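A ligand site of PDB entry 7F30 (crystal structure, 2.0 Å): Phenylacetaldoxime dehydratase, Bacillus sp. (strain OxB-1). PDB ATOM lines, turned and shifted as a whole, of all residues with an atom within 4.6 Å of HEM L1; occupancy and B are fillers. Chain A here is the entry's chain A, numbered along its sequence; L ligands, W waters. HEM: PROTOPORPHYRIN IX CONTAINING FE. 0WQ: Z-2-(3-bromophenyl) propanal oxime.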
ATOM      1  N   LEU A 128     -24.889   0.587  15.854  1.00  0.00           N
ATOM      2  CA  LEU A 128     -23.847  -0.306  16.331  1.00  0.00           C
ATOM      3  C   LEU A 128     -22.566   0.512  16.486  1.00  0.00           C
ATOM      4  O   LEU A 128     -22.232   1.315  15.612  1.00  0.00           O
ATOM      5  CB  LEU A 128     -23.612  -1.481  15.370  1.00  0.00           C
ATOM      6  CG  LEU A 128     -22.820  -2.629  15.991  1.00  0.00           C
ATOM      7  CD1 LEU A 128     -23.634  -3.307  17.106  1.00  0.00           C
ATOM      8  CD2 LEU A 128     -22.379  -3.617  14.918  1.00  0.00           C
ATOM      9  N   HIS A 150     -24.272  -8.746  17.306  1.00  0.00           N
ATOM     10  CA  HIS A 150     -23.429  -8.282  16.204  1.00  0.00           C
ATOM     11  C   HIS A 150     -22.502  -9.428  15.838  1.00  0.00           C
ATOM     12  O   HIS A 150     -22.504 -10.483  16.480  1.00  0.00           O
ATOM     13  CB  HIS A 150     -22.654  -7.016  16.599  1.00  0.00           C
ATOM     14  CG  HIS A 150     -21.540  -7.274  17.559  1.00  0.00           C
ATOM     15  ND1 HIS A 150     -20.217  -7.260  17.172  1.00  0.00           N
ATOM     16  CD2 HIS A 150     -21.543  -7.566  18.878  1.00  0.00           C
ATOM     17  CE1 HIS A 150     -19.453  -7.510  18.226  1.00  0.00           C
ATOM     18  NE2 HIS A 150     -20.241  -7.705  19.270  1.00  0.00           N
ATOM     19  N   GLU A 151     -21.683  -9.196  14.796  1.00  0.00           N
ATOM     20  CA  GLU A 151     -20.656 -10.138  14.378  1.00  0.00           C
ATOM     21  C   GLU A 151     -21.242 -11.380  13.715  1.00  0.00           C
ATOM     22  O   GLU A 151     -20.712 -12.481  13.846  1.00  0.00           O
ATOM     23  CB  GLU A 151     -19.748 -10.538  15.551  1.00  0.00           C
ATOM     24  CG  GLU A 151     -18.256 -10.424  15.281  1.00  0.00           C
ATOM     25  CD  GLU A 151     -17.430 -10.867  16.471  1.00  0.00           C
ATOM     26  OE1 GLU A 151     -17.291 -12.086  16.687  1.00  0.00           O
ATOM     27  OE2 GLU A 151     -16.941 -10.002  17.227  1.00  0.00           O
ATOM     28  N   TYR A 152     -22.367 -11.203  13.027  1.00  0.00           N
ATOM     29  CA  TYR A 152     -22.880 -12.219  12.122  1.00  0.00           C
ATOM     30  C   TYR A 152     -23.722 -11.520  11.077  1.00  0.00           C
ATOM     31  O   TYR A 152     -24.298 -10.462  11.326  1.00  0.00           O
ATOM     32  CB  TYR A 152     -23.676 -13.304  12.853  1.00  0.00           C
ATOM     33  CG  TYR A 152     -24.943 -12.836  13.567  1.00  0.00           C
ATOM     34  CD1 TYR A 152     -26.167 -12.792  12.912  1.00  0.00           C
ATOM     35  CD2 TYR A 152     -24.911 -12.458  14.901  1.00  0.00           C
ATOM     36  CE1 TYR A 152     -27.324 -12.382  13.571  1.00  0.00           C
ATOM     37  CE2 TYR A 152     -26.058 -12.019  15.569  1.00  0.00           C
ATOM     38  CZ  TYR A 152     -27.261 -11.986  14.893  1.00  0.00           C
ATOM     39  OH  TYR A 152     -28.418 -11.576  15.552  1.00  0.00           O
ATOM     40  N   TRP A 153     -23.773 -12.115   9.896  1.00  0.00           N
ATOM     41  CA  TRP A 153     -24.616 -11.585   8.844  1.00  0.00           C
ATOM     42  C   TRP A 153     -26.067 -11.749   9.234  1.00  0.00           C
ATOM     43  O   TRP A 153     -26.511 -12.858   9.553  1.00  0.00           O
ATOM     44  CB  TRP A 153     -24.334 -12.316   7.528  1.00  0.00           C
ATOM     45  CG  TRP A 153     -22.963 -12.103   6.890  1.00  0.00           C
ATOM     46  CD1 TRP A 153     -22.366 -12.953   6.006  1.00  0.00           C
ATOM     47  CD2 TRP A 153     -22.051 -10.979   7.043  1.00  0.00           C
ATOM     48  NE1 TRP A 153     -21.152 -12.446   5.607  1.00  0.00           N
ATOM     49  CE2 TRP A 153     -20.938 -11.237   6.226  1.00  0.00           C
ATOM     50  CE3 TRP A 153     -22.084  -9.793   7.779  1.00  0.00           C
ATOM     51  CZ2 TRP A 153     -19.856 -10.358   6.121  1.00  0.00           C
ATOM     52  CZ3 TRP A 153     -21.003  -8.915   7.688  1.00  0.00           C
ATOM     53  CH2 TRP A 153     -19.907  -9.211   6.854  1.00  0.00           C
ATOM     54  N   GLY A 154     -26.822 -10.661   9.201  1.00  0.00           N
ATOM     55  CA  GLY A 154     -28.173 -10.629   9.716  1.00  0.00           C
ATOM     56  C   GLY A 154     -28.296  -9.924  11.058  1.00  0.00           C
ATOM     57  O   GLY A 154     -29.428  -9.709  11.519  1.00  0.00           O
ATOM     58  N   ALA A 155     -27.190  -9.574  11.697  1.00  0.00           N
ATOM     59  CA  ALA A 155     -27.259  -8.924  12.996  1.00  0.00           C
ATOM     60  C   ALA A 155     -27.922  -7.560  12.900  1.00  0.00           C
ATOM     61  O   ALA A 155     -28.741  -7.200  13.748  1.00  0.00           O
ATOM     62  CB  ALA A 155     -25.861  -8.801  13.608  1.00  0.00           C
ATOM     63  N   MET A 156     -27.584  -6.790  11.855  1.00  0.00           N
ATOM     64  CA  MET A 156     -28.214  -5.494  11.637  1.00  0.00           C
ATOM     65  C   MET A 156     -29.732  -5.632  11.600  1.00  0.00           C
ATOM     66  O   MET A 156     -30.451  -4.925  12.332  1.00  0.00           O
ATOM     67  CB  MET A 156     -27.710  -4.868  10.323  1.00  0.00           C
ATOM     68  CG  MET A 156     -28.639  -3.781   9.766  1.00  0.00           C
ATOM     69  SD  MET A 156     -28.156  -3.099   8.163  1.00  0.00           S
ATOM     70  CE  MET A 156     -28.136  -4.595   7.180  1.00  0.00           C
ATOM     71  N   ILE A 200     -28.321   4.205   5.531  1.00  0.00           N
ATOM     72  CA  ILE A 200     -27.209   3.889   6.418  1.00  0.00           C
ATOM     73  C   ILE A 200     -26.267   5.075   6.484  1.00  0.00           C
ATOM     74  O   ILE A 200     -25.925   5.673   5.453  1.00  0.00           O
ATOM     75  CB  ILE A 200     -26.472   2.593   6.003  1.00  0.00           C
ATOM     76  CG1 ILE A 200     -25.381   2.263   7.030  1.00  0.00           C
ATOM     77  CG2 ILE A 200     -25.901   2.685   4.570  1.00  0.00           C
ATOM     78  CD1 ILE A 200     -24.619   0.987   6.759  1.00  0.00           C
ATOM     79  N   THR A 202     -22.620   5.072   7.872  1.00  0.00           N
ATOM     80  CA  THR A 202     -21.584   4.224   8.472  1.00  0.00           C
ATOM     81  C   THR A 202     -20.276   4.985   8.498  1.00  0.00           C
ATOM     82  O   THR A 202     -19.828   5.503   7.468  1.00  0.00           O
ATOM     83  CB  THR A 202     -21.458   2.889   7.741  1.00  0.00           C
ATOM     84  OG1 THR A 202     -20.385   2.128   8.317  1.00  0.00           O
ATOM     85  CG2 THR A 202     -21.225   3.076   6.249  1.00  0.00           C
ATOM     86  N   GLN A 204     -16.290   6.256  10.152  1.00  0.00           N
ATOM     87  CA  GLN A 204     -14.913   5.911  10.488  1.00  0.00           C
ATOM     88  C   GLN A 204     -14.272   7.085  11.200  1.00  0.00           C
ATOM     89  O   GLN A 204     -14.403   8.233  10.762  1.00  0.00           O
ATOM     90  CB  GLN A 204     -14.085   5.558   9.238  1.00  0.00           C
ATOM     91  CG  GLN A 204     -14.716   4.555   8.279  1.00  0.00           C
ATOM     92  CD  GLN A 204     -15.899   5.134   7.506  1.00  0.00           C
ATOM     93  OE1 GLN A 204     -15.845   6.276   7.032  1.00  0.00           O
ATOM     94  NE2 GLN A 204     -16.970   4.364   7.397  1.00  0.00           N
ATOM     95  N   TYR A 217      -4.537   2.523   8.803  1.00  0.00           N
ATOM     96  CA  TYR A 217      -5.873   2.871   8.319  1.00  0.00           C
ATOM     97  C   TYR A 217      -5.805   3.619   6.986  1.00  0.00           C
ATOM     98  O   TYR A 217      -6.507   3.276   6.031  1.00  0.00           O
ATOM     99  CB  TYR A 217      -6.646   3.701   9.337  1.00  0.00           C
ATOM    100  CG  TYR A 217      -8.008   4.046   8.753  1.00  0.00           C
ATOM    101  CD1 TYR A 217      -9.035   3.098   8.729  1.00  0.00           C
ATOM    102  CD2 TYR A 217      -8.253   5.292   8.186  1.00  0.00           C
ATOM    103  CE1 TYR A 217     -10.260   3.389   8.163  1.00  0.00           C
ATOM    104  CE2 TYR A 217      -9.470   5.592   7.627  1.00  0.00           C
ATOM    105  CZ  TYR A 217     -10.477   4.641   7.612  1.00  0.00           C
ATOM    106  OH  TYR A 217     -11.692   4.952   7.039  1.00  0.00           O
ATOM    107  N   VAL A 221      -6.706   0.462   4.651  1.00  0.00           N
ATOM    108  CA  VAL A 221      -8.154   0.300   4.779  1.00  0.00           C
ATOM    109  C   VAL A 221      -8.907   1.361   4.001  1.00  0.00           C
ATOM    110  O   VAL A 221      -9.783   1.048   3.196  1.00  0.00           O
ATOM    111  CB  VAL A 221      -8.569   0.301   6.272  1.00  0.00           C
ATOM    112  CG1 VAL A 221     -10.065   0.092   6.424  1.00  0.00           C
ATOM    113  CG2 VAL A 221      -7.780  -0.763   7.044  1.00  0.00           C
ATOM    114  N   LEU A 225     -12.324   1.477   1.210  1.00  0.00           N
ATOM    115  CA  LEU A 225     -13.554   2.225   1.434  1.00  0.00           C
ATOM    116  C   LEU A 225     -13.836   3.160   0.258  1.00  0.00           C
ATOM    117  O   LEU A 225     -14.965   3.209  -0.251  1.00  0.00           O
ATOM    118  CB  LEU A 225     -13.461   3.012   2.738  1.00  0.00           C
ATOM    119  CG  LEU A 225     -14.631   3.928   3.135  1.00  0.00           C
ATOM    120  CD1 LEU A 225     -15.921   3.126   3.292  1.00  0.00           C
ATOM    121  CD2 LEU A 225     -14.323   4.725   4.406  1.00  0.00           C
ATOM    122  N   ALA A 228     -15.075   1.044  -2.599  1.00  0.00           N
ATOM    123  CA  ALA A 228     -16.443   0.569  -2.382  1.00  0.00           C
ATOM    124  C   ALA A 228     -17.459   1.644  -2.709  1.00  0.00           C
ATOM    125  O   ALA A 228     -18.453   1.396  -3.395  1.00  0.00           O
ATOM    126  CB  ALA A 228     -16.602   0.105  -0.927  1.00  0.00           C
ATOM    127  N   LEU A 232     -20.412   1.670  -5.585  1.00  0.00           N
ATOM    128  CA  LEU A 232     -21.816   1.897  -5.269  1.00  0.00           C
ATOM    129  C   LEU A 232     -22.382   3.024  -6.115  1.00  0.00           C
ATOM    130  O   LEU A 232     -23.462   2.891  -6.708  1.00  0.00           O
ATOM    131  CB  LEU A 232     -21.983   2.186  -3.776  1.00  0.00           C
ATOM    132  CG  LEU A 232     -21.754   0.958  -2.891  1.00  0.00           C
ATOM    133  CD1 LEU A 232     -21.505   1.341  -1.441  1.00  0.00           C
ATOM    134  CD2 LEU A 232     -22.937  -0.012  -2.992  1.00  0.00           C
ATOM    135  N   VAL A 262     -19.800   7.123   5.178  1.00  0.00           N
ATOM    136  CA  VAL A 262     -20.523   6.906   3.930  1.00  0.00           C
ATOM    137  C   VAL A 262     -21.997   7.009   4.266  1.00  0.00           C
ATOM    138  O   VAL A 262     -22.457   6.414   5.243  1.00  0.00           O
ATOM    139  CB  VAL A 262     -20.190   5.546   3.305  1.00  0.00           C
ATOM    140  CG1 VAL A 262     -21.146   5.245   2.165  1.00  0.00           C
ATOM    141  CG2 VAL A 262     -18.765   5.547   2.794  1.00  0.00           C
ATOM    142  N   TYR A 266     -30.626   2.725  -0.046  1.00  0.00           N
ATOM    143  CA  TYR A 266     -30.807   1.457  -0.758  1.00  0.00           C
ATOM    144  C   TYR A 266     -32.292   1.182  -0.927  1.00  0.00           C
ATOM    145  O   TYR A 266     -33.110   1.623  -0.111  1.00  0.00           O
ATOM    146  CB  TYR A 266     -30.120   0.293  -0.001  1.00  0.00           C
ATOM    147  CG  TYR A 266     -28.624   0.413   0.027  1.00  0.00           C
ATOM    148  CD1 TYR A 266     -27.987   1.299   0.882  1.00  0.00           C
ATOM    149  CD2 TYR A 266     -27.834  -0.336  -0.831  1.00  0.00           C
ATOM    150  CE1 TYR A 266     -26.611   1.421   0.899  1.00  0.00           C
ATOM    151  CE2 TYR A 266     -26.445  -0.225  -0.829  1.00  0.00           C
ATOM    152  CZ  TYR A 266     -25.843   0.665   0.033  1.00  0.00           C
ATOM    153  OH  TYR A 266     -24.473   0.788   0.027  1.00  0.00           O
ATOM    154  N   LEU A 272     -28.885  -3.708   0.750  1.00  0.00           N
ATOM    155  CA  LEU A 272     -27.725  -3.391   1.552  1.00  0.00           C
ATOM    156  C   LEU A 272     -27.069  -4.663   2.091  1.00  0.00           C
ATOM    157  O   LEU A 272     -25.845  -4.816   2.048  1.00  0.00           O
ATOM    158  CB  LEU A 272     -28.123  -2.450   2.688  1.00  0.00           C
ATOM    159  CG  LEU A 272     -27.113  -2.113   3.797  1.00  0.00           C
ATOM    160  CD1 LEU A 272     -25.846  -1.482   3.229  1.00  0.00           C
ATOM    161  CD2 LEU A 272     -27.723  -1.198   4.825  1.00  0.00           C
ATOM    162  N   TRP A 275     -25.209  -6.680  -0.704  1.00  0.00           N
ATOM    163  CA  TRP A 275     -23.947  -6.028  -1.074  1.00  0.00           C
ATOM    164  C   TRP A 275     -22.912  -6.264   0.004  1.00  0.00           C
ATOM    165  O   TRP A 275     -21.774  -6.659  -0.294  1.00  0.00           O
ATOM    166  CB  TRP A 275     -24.158  -4.529  -1.310  1.00  0.00           C
ATOM    167  CG  TRP A 275     -22.846  -3.835  -1.584  1.00  0.00           C
ATOM    168  CD1 TRP A 275     -22.186  -3.771  -2.788  1.00  0.00           C
ATOM    169  CD2 TRP A 275     -22.025  -3.151  -0.638  1.00  0.00           C
ATOM    170  NE1 TRP A 275     -20.996  -3.086  -2.635  1.00  0.00           N
ATOM    171  CE2 TRP A 275     -20.877  -2.694  -1.324  1.00  0.00           C
ATOM    172  CE3 TRP A 275     -22.133  -2.891   0.729  1.00  0.00           C
ATOM    173  CZ2 TRP A 275     -19.858  -1.984  -0.695  1.00  0.00           C
ATOM    174  CZ3 TRP A 275     -21.108  -2.192   1.365  1.00  0.00           C
ATOM    175  CH2 TRP A 275     -19.995  -1.741   0.655  1.00  0.00           C
ATOM    176  N   THR A 276     -23.283  -6.036   1.267  1.00  0.00           N
ATOM    177  CA  THR A 276     -22.330  -6.154   2.355  1.00  0.00           C
ATOM    178  C   THR A 276     -21.817  -7.576   2.499  1.00  0.00           C
ATOM    179  O   THR A 276     -20.624  -7.791   2.763  1.00  0.00           O
ATOM    180  CB  THR A 276     -22.960  -5.714   3.680  1.00  0.00           C
ATOM    181  OG1 THR A 276     -23.528  -4.417   3.529  1.00  0.00           O
ATOM    182  CG2 THR A 276     -21.894  -5.683   4.779  1.00  0.00           C
ATOM    183  N   HIS A 277     -22.694  -8.563   2.346  1.00  0.00           N
ATOM    184  CA  HIS A 277     -22.323  -9.947   2.600  1.00  0.00           C
ATOM    185  C   HIS A 277     -21.625 -10.591   1.403  1.00  0.00           C
ATOM    186  O   HIS A 277     -20.752 -11.435   1.593  1.00  0.00           O
ATOM    187  CB  HIS A 277     -23.552 -10.782   2.942  1.00  0.00           C
ATOM    188  CG  HIS A 277     -24.331 -10.259   4.102  1.00  0.00           C
ATOM    189  ND1 HIS A 277     -25.656 -10.577   4.313  1.00  0.00           N
ATOM    190  CD2 HIS A 277     -23.977  -9.445   5.127  1.00  0.00           C
ATOM    191  CE1 HIS A 277     -26.086  -9.984   5.419  1.00  0.00           C
ATOM    192  NE2 HIS A 277     -25.078  -9.288   5.934  1.00  0.00           N
ATOM    193  N   HIS A 282     -17.075  -4.777  -0.272  1.00  0.00           N
ATOM    194  CA  HIS A 282     -17.112  -4.780   1.185  1.00  0.00           C
ATOM    195  C   HIS A 282     -16.258  -5.892   1.767  1.00  0.00           C
ATOM    196  O   HIS A 282     -15.729  -5.751   2.884  1.00  0.00           O
ATOM    197  CB  HIS A 282     -18.536  -4.902   1.720  1.00  0.00           C
ATOM    198  CG  HIS A 282     -18.619  -4.711   3.205  1.00  0.00           C
ATOM    199  ND1 HIS A 282     -18.493  -5.749   4.101  1.00  0.00           N
ATOM    200  CD2 HIS A 282     -18.765  -3.585   3.940  1.00  0.00           C
ATOM    201  CE1 HIS A 282     -18.591  -5.273   5.335  1.00  0.00           C
ATOM    202  NE2 HIS A 282     -18.748  -3.969   5.271  1.00  0.00           N
ATOM    203  N   ILE A 285     -12.943  -4.504   2.223  1.00  0.00           N
ATOM    204  CA  ILE A 285     -12.937  -3.633   3.401  1.00  0.00           C
ATOM    205  C   ILE A 285     -12.775  -4.460   4.661  1.00  0.00           C
ATOM    206  O   ILE A 285     -11.905  -4.197   5.492  1.00  0.00           O
ATOM    207  CB  ILE A 285     -14.233  -2.811   3.477  1.00  0.00           C
ATOM    208  CG1 ILE A 285     -14.345  -1.785   2.361  1.00  0.00           C
ATOM    209  CG2 ILE A 285     -14.306  -2.121   4.799  1.00  0.00           C
ATOM    210  CD1 ILE A 285     -15.683  -1.030   2.440  1.00  0.00           C
ATOM    211  N   TYR A 286     -13.651  -5.461   4.833  1.00  0.00           N
ATOM    212  CA  TYR A 286     -13.576  -6.326   6.004  1.00  0.00           C
ATOM    213  C   TYR A 286     -12.200  -7.001   6.078  1.00  0.00           C
ATOM    214  O   TYR A 286     -11.606  -7.086   7.160  1.00  0.00           O
ATOM    215  CB  TYR A 286     -14.710  -7.354   5.959  1.00  0.00           C
ATOM    216  CG  TYR A 286     -15.041  -8.037   7.284  1.00  0.00           C
ATOM    217  CD1 TYR A 286     -14.112  -8.867   7.916  1.00  0.00           C
ATOM    218  CD2 TYR A 286     -16.290  -7.877   7.872  1.00  0.00           C
ATOM    219  CE1 TYR A 286     -14.405  -9.487   9.118  1.00  0.00           C
ATOM    220  CE2 TYR A 286     -16.606  -8.505   9.080  1.00  0.00           C
ATOM    221  CZ  TYR A 286     -15.652  -9.306   9.693  1.00  0.00           C
ATOM    222  OH  TYR A 286     -15.938  -9.937  10.888  1.00  0.00           O
ATOM    223  N   PHE A 289      -9.584  -4.493   7.206  1.00  0.00           N
ATOM    224  CA  PHE A 289      -9.811  -4.194   8.620  1.00  0.00           C
ATOM    225  C   PHE A 289      -9.228  -5.284   9.496  1.00  0.00           C
ATOM    226  O   PHE A 289      -8.503  -5.004  10.464  1.00  0.00           O
ATOM    227  CB  PHE A 289     -11.304  -4.026   8.887  1.00  0.00           C
ATOM    228  CG  PHE A 289     -11.637  -3.780  10.336  1.00  0.00           C
ATOM    229  CD1 PHE A 289     -11.076  -2.708  11.027  1.00  0.00           C
ATOM    230  CD2 PHE A 289     -12.521  -4.603  11.018  1.00  0.00           C
ATOM    231  CE1 PHE A 289     -11.370  -2.479  12.356  1.00  0.00           C
ATOM    232  CE2 PHE A 289     -12.837  -4.373  12.354  1.00  0.00           C
ATOM    233  CZ  PHE A 289     -12.254  -3.302  13.024  1.00  0.00           C
ATOM    234  N   LEU A 302      -9.187   2.841  16.433  1.00  0.00           N
ATOM    235  CA  LEU A 302     -10.133   3.189  15.384  1.00  0.00           C
ATOM    236  C   LEU A 302     -11.561   3.008  15.887  1.00  0.00           C
ATOM    237  O   LEU A 302     -11.915   1.942  16.402  1.00  0.00           O
ATOM    238  CB  LEU A 302      -9.903   2.318  14.152  1.00  0.00           C
ATOM    239  CG  LEU A 302     -10.795   2.578  12.931  1.00  0.00           C
ATOM    240  CD1 LEU A 302     -10.515   3.957  12.334  1.00  0.00           C
ATOM    241  CD2 LEU A 302     -10.606   1.492  11.887  1.00  0.00           C
ATOM    242  N   LEU A 304     -15.498   2.798  14.889  1.00  0.00           N
ATOM    243  CA  LEU A 304     -16.458   2.555  13.829  1.00  0.00           C
ATOM    244  C   LEU A 304     -17.852   2.538  14.418  1.00  0.00           C
ATOM    245  O   LEU A 304     -18.061   2.103  15.567  1.00  0.00           O
ATOM    246  CB  LEU A 304     -16.168   1.233  13.111  1.00  0.00           C
ATOM    247  CG  LEU A 304     -14.791   1.114  12.452  1.00  0.00           C
ATOM    248  CD1 LEU A 304     -14.483  -0.318  12.142  1.00  0.00           C
ATOM    249  CD2 LEU A 304     -14.725   1.940  11.186  1.00  0.00           C
ATOM    250  N   HIS A 306     -22.379   2.756  12.983  1.00  0.00           N
ATOM    251  CA  HIS A 306     -23.341   3.104  11.947  1.00  0.00           C
ATOM    252  C   HIS A 306     -24.721   3.307  12.539  1.00  0.00           C
ATOM    253  O   HIS A 306     -25.024   2.842  13.648  1.00  0.00           O
ATOM    254  CB  HIS A 306     -23.341   2.081  10.799  1.00  0.00           C
ATOM    255  CG  HIS A 306     -24.070   0.799  11.071  1.00  0.00           C
ATOM    256  ND1 HIS A 306     -23.827  -0.347  10.353  1.00  0.00           N
ATOM    257  CD2 HIS A 306     -25.075   0.482  11.932  1.00  0.00           C
ATOM    258  CE1 HIS A 306     -24.622  -1.307  10.770  1.00  0.00           C
ATOM    259  NE2 HIS A 306     -25.392  -0.836  11.723  1.00  0.00           N
HETATM  260  CHA HEM L   1     -20.854  -4.777   9.015  1.00  0.00           C
HETATM  261  CHB HEM L   1     -22.193  -1.793   5.419  1.00  0.00           C
HETATM  262  CHC HEM L   1     -17.780   0.270   5.578  1.00  0.00           C
HETATM  263  CHD HEM L   1     -16.302  -3.146   8.673  1.00  0.00           C
HETATM  264  C1A HEM L   1     -21.622  -4.070   8.108  1.00  0.00           C
HETATM  265  C2A HEM L   1     -23.069  -4.169   7.955  1.00  0.00           C
HETATM  266  C3A HEM L   1     -23.425  -3.347   6.970  1.00  0.00           C
HETATM  267  C4A HEM L   1     -22.237  -2.700   6.449  1.00  0.00           C
HETATM  268  CMA HEM L   1     -24.864  -3.118   6.456  1.00  0.00           C
HETATM  269  CAA HEM L   1     -24.029  -5.053   8.809  1.00  0.00           C
HETATM  270  CBA HEM L   1     -24.301  -6.383   8.105  1.00  0.00           C
HETATM  271  CGA HEM L   1     -25.155  -7.259   8.998  1.00  0.00           C
HETATM  272  O1A HEM L   1     -25.899  -8.109   8.451  1.00  0.00           O
HETATM  273  O2A HEM L   1     -25.119  -7.088  10.246  1.00  0.00           O
HETATM  274  C1B HEM L   1     -21.116  -0.975   5.120  1.00  0.00           C
HETATM  275  C2B HEM L   1     -21.062   0.032   4.081  1.00  0.00           C
HETATM  276  C3B HEM L   1     -19.837   0.608   4.160  1.00  0.00           C
HETATM  277  C4B HEM L   1     -19.076  -0.044   5.203  1.00  0.00           C
HETATM  278  CMB HEM L   1     -22.246   0.397   3.143  1.00  0.00           C
HETATM  279  CAB HEM L   1     -19.210   1.734   3.304  1.00  0.00           C
HETATM  280  CBB HEM L   1     -19.550   1.945   2.031  1.00  0.00           C
HETATM  281  C1C HEM L   1     -16.987  -0.399   6.495  1.00  0.00           C
HETATM  282  C2C HEM L   1     -15.655  -0.033   6.980  1.00  0.00           C
HETATM  283  C3C HEM L   1     -15.264  -0.993   7.833  1.00  0.00           C
HETATM  284  C4C HEM L   1     -16.328  -1.984   7.920  1.00  0.00           C
HETATM  285  CMC HEM L   1     -14.851   1.228   6.554  1.00  0.00           C
HETATM  286  CAC HEM L   1     -13.947  -1.133   8.622  1.00  0.00           C
HETATM  287  CBC HEM L   1     -12.880  -0.342   8.492  1.00  0.00           C
HETATM  288  C1D HEM L   1     -17.381  -3.897   9.052  1.00  0.00           C
HETATM  289  C2D HEM L   1     -17.430  -4.934  10.069  1.00  0.00           C
HETATM  290  C3D HEM L   1     -18.698  -5.373  10.157  1.00  0.00           C
HETATM  291  C4D HEM L   1     -19.498  -4.641   9.215  1.00  0.00           C
HETATM  292  CMD HEM L   1     -16.237  -5.456  10.908  1.00  0.00           C
HETATM  293  CAD HEM L   1     -19.225  -6.453  11.118  1.00  0.00           C
HETATM  294  CBD HEM L   1     -19.815  -5.647  12.291  1.00  0.00           C
HETATM  295  CGD HEM L   1     -20.416  -6.486  13.394  1.00  0.00           C
HETATM  296  O1D HEM L   1     -19.730  -6.658  14.433  1.00  0.00           O
HETATM  297  O2D HEM L   1     -21.566  -6.964  13.244  1.00  0.00           O
HETATM  298  NA  HEM L   1     -21.148  -3.167   7.173  1.00  0.00           N
HETATM  299  NB  HEM L   1     -19.897  -0.998   5.768  1.00  0.00           N
HETATM  300  NC  HEM L   1     -17.342  -1.589   7.090  1.00  0.00           N
HETATM  301  ND  HEM L   1     -18.665  -3.754   8.548  1.00  0.00           N
HETATM  302 FE   HEM L   1     -19.238  -2.485   7.042  1.00  0.00          FE
HETATM  303  C11 0WQ L   2     -16.470  -2.771  12.684  1.00  0.00           C
HETATM  304  C10 0WQ L   2     -16.753  -3.105  13.983  1.00  0.00           C
HETATM  305  C12 0WQ L   2     -17.430  -2.181  11.856  1.00  0.00           C
HETATM  306  C01 0WQ L   2     -20.204  -0.004  12.151  1.00  0.00           C
HETATM  307  C02 0WQ L   2     -19.753  -1.281  11.443  1.00  0.00           C
HETATM  308  C03 0WQ L   2     -19.226  -1.044  10.014  1.00  0.00           C
HETATM  309  C06 0WQ L   2     -18.694  -1.923  12.335  1.00  0.00           C
HETATM  310  C07 0WQ L   2     -18.990  -2.237  13.649  1.00  0.00           C
HETATM  311  C08 0WQ L   2     -18.022  -2.826  14.441  1.00  0.00           C
HETATM  312  N04 0WQ L   2     -19.915  -0.662   9.019  1.00  0.00           N
HETATM  313  O05 0WQ L   2     -21.294  -0.345   9.077  1.00  0.00           O
HETATM  314 BR9  0WQ L   2     -18.436  -3.293  16.268  1.00  0.00          BR
HETATM  315  O   HOH W   1     -28.557  -7.649   8.672  1.00  0.00           O
HETATM  316  O   HOH W   2     -24.097  -5.785  12.416  1.00  0.00           O
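A ring nitrogen (NE2) of His 282 binds an iron atom (FE) of HEM L1 (2.4 Å). The backbone NH of Glu 151 is in hydrogen-bond range of an oxygen (O2D) of HEM L1, 2.7 Å away. An oxygen (O1A) of HEM L1 is in hydrogen-bond range of the backbone NH (N) of Gly 154 (2.8 Å). An oxygen (O1D) of HEM L1 lies within hydrogen-bond range of a ring nitrogen (ND1) of His 150, at 2.8 Å. O1A of HEM L1 sits at hydrogen-bond distance from NE2 of His 277 (2.9 Å). N of Met 156 sits at hydrogen-bond distance from O2A of HEM L1 (3.0 Å). The side-chain hydroxyl (OG1) of Thr 202 is in hydrogen-bond range of an oxygen (O05) of 0WQ L2 (2.7 Å). ND1 of His 306 lies within hydrogen-bond range of O05 of 0WQ L2, 2.8 Å away.
ND1 of His 282 sits at hydrogen-bond distance from O of Thr 276 (3.2 Å). The side-chain hydroxyl of Thr 276 lies within hydrogen-bond range of the backbone carbonyl oxygen of Leu 272. O of Thr 202 sits at hydrogen-bond distance from N of Val 262 (2.8 Å). The side-chain amide nitrogen (NE2) of Gln 204 sits at hydrogen-bond distance from the backbone carbonyl oxygen (O) of Thr 202 (3.1 Å). N of His 306 is in hydrogen-bond range of O of Leu 128 (3.0 Å).
Leu 128 touches HEM L1 (CD2 to CGD, 3.8 Å). Tyr 152 touches HEM L1. CA of Trp 153 touches O1A of HEM L1, at 3.7 Å. Ala 155 touches HEM L1 (N to O2A, 3.5 Å). CD1 of Ile 200 touches CHB of HEM L1, 3.9 Å away. Thr 202 touches HEM L1. Gln 204 touches HEM L1. Val 221 touches HEM L1. Leu 225 touches HEM L1. Val 262 touches HEM L1. Tyr 266 touches HEM L1 (OH to CMB, 3.8 Å). Leu 272 touches HEM L1. Trp 275 touches HEM L1. Thr 276 touches HEM L1. Ile 285 touches HEM L1. Tyr 286 touches HEM L1. Phe 289 touches HEM L1 (CD2 to CMD, 3.8 Å). CD1 of Leu 304 touches CAC of HEM L1, at 3.7 Å. Hydrophobic or aromatic side chains within 4 Å of HEM L1: Leu 128, His 150, Ala 155, Met 156, Ile 200, Val 221, Leu 225, Val 262, Leu 272, Trp 275, His 277, His 282, Ile 285, Tyr 286, Phe 289 and Leu 304. Within 4 Å of HEM L1: Leu 128, His 150, Glu 151, Tyr 152, Trp 153, Gly 154, Ala 155, Met 156, Ile 200, Thr 202, Gln 204, Val 221, Leu 225, Val 262, Tyr 266, Leu 272, Trp 275, Thr 276, His 277, His 282, Ile 285, Tyr 286, Phe 289 and Leu 304. The nearest printed residue that does not touch HEM L1 is Leu 232 (4.03 Å).
Water W1 bridges O1A of HEM L1 (2.7 Å) and N of Met 156 (3.4 Å).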
